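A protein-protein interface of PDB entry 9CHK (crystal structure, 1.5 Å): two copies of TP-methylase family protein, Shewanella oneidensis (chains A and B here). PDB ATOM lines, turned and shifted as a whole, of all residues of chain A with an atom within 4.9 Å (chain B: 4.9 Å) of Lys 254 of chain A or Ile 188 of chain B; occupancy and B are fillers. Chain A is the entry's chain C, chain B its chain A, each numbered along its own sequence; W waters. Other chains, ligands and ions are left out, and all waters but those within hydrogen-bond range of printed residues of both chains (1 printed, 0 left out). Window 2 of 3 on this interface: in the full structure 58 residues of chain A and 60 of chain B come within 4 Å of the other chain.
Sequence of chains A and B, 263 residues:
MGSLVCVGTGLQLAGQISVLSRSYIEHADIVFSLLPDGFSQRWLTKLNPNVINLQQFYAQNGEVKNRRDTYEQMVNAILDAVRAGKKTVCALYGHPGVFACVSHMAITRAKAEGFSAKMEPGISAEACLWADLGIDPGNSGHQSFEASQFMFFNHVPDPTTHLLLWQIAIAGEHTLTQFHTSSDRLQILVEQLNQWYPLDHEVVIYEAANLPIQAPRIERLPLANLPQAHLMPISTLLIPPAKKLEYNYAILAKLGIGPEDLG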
ATOM      1  N   ALA A 250      32.819 -24.247  16.968  1.00  0.00           N
ATOM      2  CA  ALA A 250      31.496 -24.159  16.373  1.00  0.00           C
ATOM      3  C   ALA A 250      31.277 -22.785  15.742  1.00  0.00           C
ATOM      4  O   ALA A 250      30.836 -22.682  14.597  1.00  0.00           O
ATOM      5  CB  ALA A 250      30.447 -24.450  17.421  1.00  0.00           C
ATOM      6  N   ILE A 251      31.582 -21.726  16.496  1.00  0.00           N
ATOM      7  CA  ILE A 251      31.280 -20.374  16.053  1.00  0.00           C
ATOM      8  C   ILE A 251      32.359 -19.901  15.079  1.00  0.00           C
ATOM      9  O   ILE A 251      32.063 -19.180  14.130  1.00  0.00           O
ATOM     10  CB  ILE A 251      31.121 -19.421  17.252  1.00  0.00           C
ATOM     11  CG1 ILE A 251      30.064 -19.922  18.251  1.00  0.00           C
ATOM     12  CG2 ILE A 251      30.831 -17.997  16.777  1.00  0.00           C
ATOM     13  CD1 ILE A 251      28.684 -20.151  17.661  1.00  0.00           C
ATOM     14  N   LEU A 252      33.611 -20.313  15.311  1.00  0.00           N
ATOM     15  CA  LEU A 252      34.688 -20.005  14.383  1.00  0.00           C
ATOM     16  C   LEU A 252      34.319 -20.543  13.002  1.00  0.00           C
ATOM     17  O   LEU A 252      34.522 -19.867  11.997  1.00  0.00           O
ATOM     18  CB  LEU A 252      36.020 -20.564  14.881  1.00  0.00           C
ATOM     19  CG  LEU A 252      36.541 -19.984  16.204  1.00  0.00           C
ATOM     20  CD1 LEU A 252      37.801 -20.715  16.641  1.00  0.00           C
ATOM     21  CD2 LEU A 252      36.803 -18.487  16.114  1.00  0.00           C
ATOM     22  N   ALA A 253      33.750 -21.753  12.964  1.00  0.00           N
ATOM     23  CA  ALA A 253      33.347 -22.368  11.709  1.00  0.00           C
ATOM     24  C   ALA A 253      32.290 -21.509  11.017  1.00  0.00           C
ATOM     25  O   ALA A 253      32.361 -21.299   9.810  1.00  0.00           O
ATOM     26  CB  ALA A 253      32.853 -23.779  11.947  1.00  0.00           C
ATOM     27  N   LYS A 254      31.314 -21.001  11.780  1.00  0.00           N
ATOM     28  CA  LYS A 254      30.267 -20.169  11.206  1.00  0.00           C
ATOM     29  C   LYS A 254      30.868 -18.879  10.646  1.00  0.00           C
ATOM     30  O   LYS A 254      30.402 -18.366   9.629  1.00  0.00           O
ATOM     31  CB  LYS A 254      29.143 -19.832  12.194  1.00  0.00           C
ATOM     32  CG  LYS A 254      27.998 -20.838  12.264  1.00  0.00           C
ATOM     33  CD  LYS A 254      28.148 -21.912  13.332  1.00  0.00           C
ATOM     34  CE  LYS A 254      27.267 -23.102  13.101  1.00  0.00           C
ATOM     35  NZ  LYS A 254      25.854 -22.851  13.394  1.00  0.00           N
ATOM     36  N   LEU A 255      31.913 -18.368  11.308  1.00  0.00           N
ATOM     37  CA  LEU A 255      32.560 -17.128  10.907  1.00  0.00           C
ATOM     38  C   LEU A 255      33.501 -17.378   9.728  1.00  0.00           C
ATOM     39  O   LEU A 255      33.978 -16.435   9.102  1.00  0.00           O
ATOM     40  CB  LEU A 255      33.306 -16.540  12.106  1.00  0.00           C
ATOM     41  CG  LEU A 255      32.436 -15.971  13.233  1.00  0.00           C
ATOM     42  CD1 LEU A 255      33.250 -15.710  14.488  1.00  0.00           C
ATOM     43  CD2 LEU A 255      31.737 -14.696  12.791  1.00  0.00           C
ATOM     44  N   GLY A 256      33.775 -18.655   9.442  1.00  0.00           N
ATOM     45  CA  GLY A 256      34.628 -19.034   8.328  1.00  0.00           C
ATOM     46  C   GLY A 256      36.111 -18.845   8.645  1.00  0.00           C
ATOM     47  O   GLY A 256      36.909 -18.616   7.740  1.00  0.00           O
ATOM     48  N   MET B 151      32.241 -15.146  21.388  1.00  0.00           N
ATOM     49  CA  MET B 151      32.080 -15.831  20.115  1.00  0.00           C
ATOM     50  C   MET B 151      33.244 -16.784  19.847  1.00  0.00           C
ATOM     51  O   MET B 151      33.032 -17.871  19.319  1.00  0.00           O
ATOM     52  CB  MET B 151      31.948 -14.826  18.967  1.00  0.00           C
ATOM     53  CG  MET B 151      30.718 -13.953  19.088  1.00  0.00           C
ATOM     54  SD  MET B 151      30.444 -12.872  17.672  1.00  0.00           S
ATOM     55  CE  MET B 151      29.782 -14.042  16.477  1.00  0.00           C
ATOM     56  N   ASP B 184      26.351  -9.578   9.344  1.00  0.00           N
ATOM     57  CA  ASP B 184      26.450 -11.025   9.238  1.00  0.00           C
ATOM     58  C   ASP B 184      27.014 -11.608  10.532  1.00  0.00           C
ATOM     59  O   ASP B 184      26.529 -12.628  11.014  1.00  0.00           O
ATOM     60  CB  ASP B 184      27.256 -11.434   8.014  1.00  0.00           C
ATOM     61  CG  ASP B 184      26.545 -11.243   6.682  1.00  0.00           C
ATOM     62  OD1 ASP B 184      25.329 -10.950   6.705  1.00  0.00           O
ATOM     63  OD2 ASP B 184      27.212 -11.380   5.634  1.00  0.00           O
ATOM     64  N   ARG B 185      28.046 -10.962  11.085  1.00  0.00           N
ATOM     65  CA  ARG B 185      28.659 -11.416  12.323  1.00  0.00           C
ATOM     66  C   ARG B 185      27.663 -11.293  13.472  1.00  0.00           C
ATOM     67  O   ARG B 185      27.598 -12.162  14.339  1.00  0.00           O
ATOM     68  CB  ARG B 185      29.929 -10.629  12.665  1.00  0.00           C
ATOM     69  CG  ARG B 185      31.226 -11.195  12.104  1.00  0.00           C
ATOM     70  CD  ARG B 185      31.527 -10.758  10.685  1.00  0.00           C
ATOM     71  NE  ARG B 185      32.970 -10.828  10.427  1.00  0.00           N
ATOM     72  CZ  ARG B 185      33.782  -9.776  10.422  1.00  0.00           C
ATOM     73  NH1 ARG B 185      35.072  -9.936  10.186  1.00  0.00           N
ATOM     74  NH2 ARG B 185      33.305  -8.568  10.664  1.00  0.00           N
ATOM     75  N   LEU B 186      26.899 -10.198  13.488  1.00  0.00           N
ATOM     76  CA  LEU B 186      25.940  -9.985  14.556  1.00  0.00           C
ATOM     77  C   LEU B 186      24.838 -11.040  14.482  1.00  0.00           C
ATOM     78  O   LEU B 186      24.342 -11.480  15.515  1.00  0.00           O
ATOM     79  CB  LEU B 186      25.402  -8.557  14.504  1.00  0.00           C
ATOM     80  CG  LEU B 186      26.374  -7.483  15.003  1.00  0.00           C
ATOM     81  CD1 LEU B 186      25.890  -6.090  14.656  1.00  0.00           C
ATOM     82  CD2 LEU B 186      26.590  -7.602  16.504  1.00  0.00           C
ATOM     83  N   GLN B 187      24.485 -11.466  13.264  1.00  0.00           N
ATOM     84  CA  GLN B 187      23.469 -12.492  13.070  1.00  0.00           C
ATOM     85  C   GLN B 187      23.950 -13.819  13.657  1.00  0.00           C
ATOM     86  O   GLN B 187      23.174 -14.560  14.257  1.00  0.00           O
ATOM     87  CB  GLN B 187      23.142 -12.616  11.580  1.00  0.00           C
ATOM     88  CG  GLN B 187      22.145 -13.717  11.235  1.00  0.00           C
ATOM     89  CD  GLN B 187      20.816 -13.579  11.946  1.00  0.00           C
ATOM     90  OE1 GLN B 187      20.293 -12.475  12.132  1.00  0.00           O
ATOM     91  NE2 GLN B 187      20.263 -14.708  12.361  1.00  0.00           N
ATOM     92  N   ILE B 188      25.241 -14.111  13.480  1.00  0.00           N
ATOM     93  CA  ILE B 188      25.830 -15.316  14.038  1.00  0.00           C
ATOM     94  C   ILE B 188      25.780 -15.240  15.563  1.00  0.00           C
ATOM     95  O   ILE B 188      25.516 -16.237  16.233  1.00  0.00           O
ATOM     96  CB  ILE B 188      27.256 -15.518  13.492  1.00  0.00           C
ATOM     97  CG1 ILE B 188      27.214 -15.886  12.006  1.00  0.00           C
ATOM     98  CG2 ILE B 188      28.026 -16.553  14.317  1.00  0.00           C
ATOM     99  CD1 ILE B 188      28.573 -15.907  11.331  1.00  0.00           C
ATOM    100  N   LEU B 189      26.024 -14.050  16.115  1.00  0.00           N
ATOM    101  CA  LEU B 189      25.951 -13.872  17.556  1.00  0.00           C
ATOM    102  C   LEU B 189      24.517 -14.110  18.028  1.00  0.00           C
ATOM    103  O   LEU B 189      24.296 -14.737  19.058  1.00  0.00           O
ATOM    104  CB  LEU B 189      26.454 -12.488  17.961  1.00  0.00           C
ATOM    105  CG  LEU B 189      26.359 -12.153  19.453  1.00  0.00           C
ATOM    106  CD1 LEU B 189      27.217 -13.075  20.303  1.00  0.00           C
ATOM    107  CD2 LEU B 189      26.741 -10.704  19.697  1.00  0.00           C
ATOM    108  N   VAL B 190      23.540 -13.599  17.272  1.00  0.00           N
ATOM    109  CA  VAL B 190      22.140 -13.778  17.623  1.00  0.00           C
ATOM    110  C   VAL B 190      21.812 -15.270  17.675  1.00  0.00           C
ATOM    111  O   VAL B 190      21.226 -15.749  18.640  1.00  0.00           O
ATOM    112  CB  VAL B 190      21.231 -13.017  16.639  1.00  0.00           C
ATOM    113  CG1 VAL B 190      19.789 -13.501  16.691  1.00  0.00           C
ATOM    114  CG2 VAL B 190      21.298 -11.515  16.876  1.00  0.00           C
ATOM    115  N   GLU B 191      22.212 -16.009  16.639  1.00  0.00           N
ATOM    116  CA  GLU B 191      21.922 -17.431  16.570  1.00  0.00           C
ATOM    117  C   GLU B 191      22.587 -18.156  17.740  1.00  0.00           C
ATOM    118  O   GLU B 191      22.015 -19.087  18.303  1.00  0.00           O
ATOM    119  CB  GLU B 191      22.366 -17.990  15.219  1.00  0.00           C
ATOM    120  CG  GLU B 191      21.524 -17.462  14.061  1.00  0.00           C
ATOM    121  CD  GLU B 191      22.014 -17.842  12.676  1.00  0.00           C
ATOM    122  OE1 GLU B 191      22.938 -18.677  12.564  1.00  0.00           O
ATOM    123  OE2 GLU B 191      21.466 -17.282  11.703  1.00  0.00           O
ATOM    124  N   GLN B 192      23.808 -17.735  18.082  1.00  0.00           N
ATOM    125  CA  GLN B 192      24.540 -18.315  19.196  1.00  0.00           C
ATOM    126  C   GLN B 192      23.772 -18.083  20.495  1.00  0.00           C
ATOM    127  O   GLN B 192      23.602 -18.998  21.298  1.00  0.00           O
ATOM    128  CB  GLN B 192      25.932 -17.694  19.311  1.00  0.00           C
ATOM    129  CG  GLN B 192      26.782 -18.285  20.432  1.00  0.00           C
ATOM    130  CD  GLN B 192      28.116 -17.593  20.610  1.00  0.00           C
ATOM    131  OE1 GLN B 192      28.347 -16.489  20.104  1.00  0.00           O
ATOM    132  NE2 GLN B 192      29.006 -18.233  21.352  1.00  0.00           N
HETATM  133  O   HOH W   1      33.784 -13.748   9.707  1.00  0.00           O
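Water W1 bridges the backbone carbonyl oxygen of Leu 255 of chain A and the guanidinium group of Arg 185 of chain B.
Hydrophobic or aromatic side chains of chain A within 4 Å of the printed part of chain B: Ile 251 and Leu 255. Hydrophobic or aromatic side chains of chain B that line the printed part of chain A: Ile 188.
Of the printed residues of chain B, Lys 254 of chain A touches Ile 188. Printed residues of chain A within 4 Å of Ile 188 of chain B: Lys 254 and Leu 255. Printed residues of chain B within 4 Å of Ile 251 of chain A: Met 151 and Gln 192. Printed residues of chain B within 4 Å of Leu 255 of chain A: Arg 185 (3.6 Å) and Ile 188 (3.7 Å). Printed residues of chain A within 4 Å of Met 151 of chain B: Ile 251 (3.2 Å). Of the printed residues of chain A, Gln 192 of chain B touches Ile 251 (3.7 Å). The nearest printed residue of chain A that does not touch Ile 188 of chain B is Ile 251 of chain A (4.001 Å).
Among the printed residues, merely in contact across the chains: Ile 251 of chain A with Met 151 of chain B (3.2 Å), Lys 254 of chain A with Ile 188 of chain B (3.5 Å), Leu 255 of chain A with Arg 185 of chain B (3.6 Å), Ile 251 of chain A with Gln 192 of chain B (3.7 Å) and Leu 255 of chain A with Ile 188 of chain B (3.7 Å).
No position is printed for both chains. Of the 5 pairs that touch across the chains among the printed residues, none has its exchanged pair printed and touching as well.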
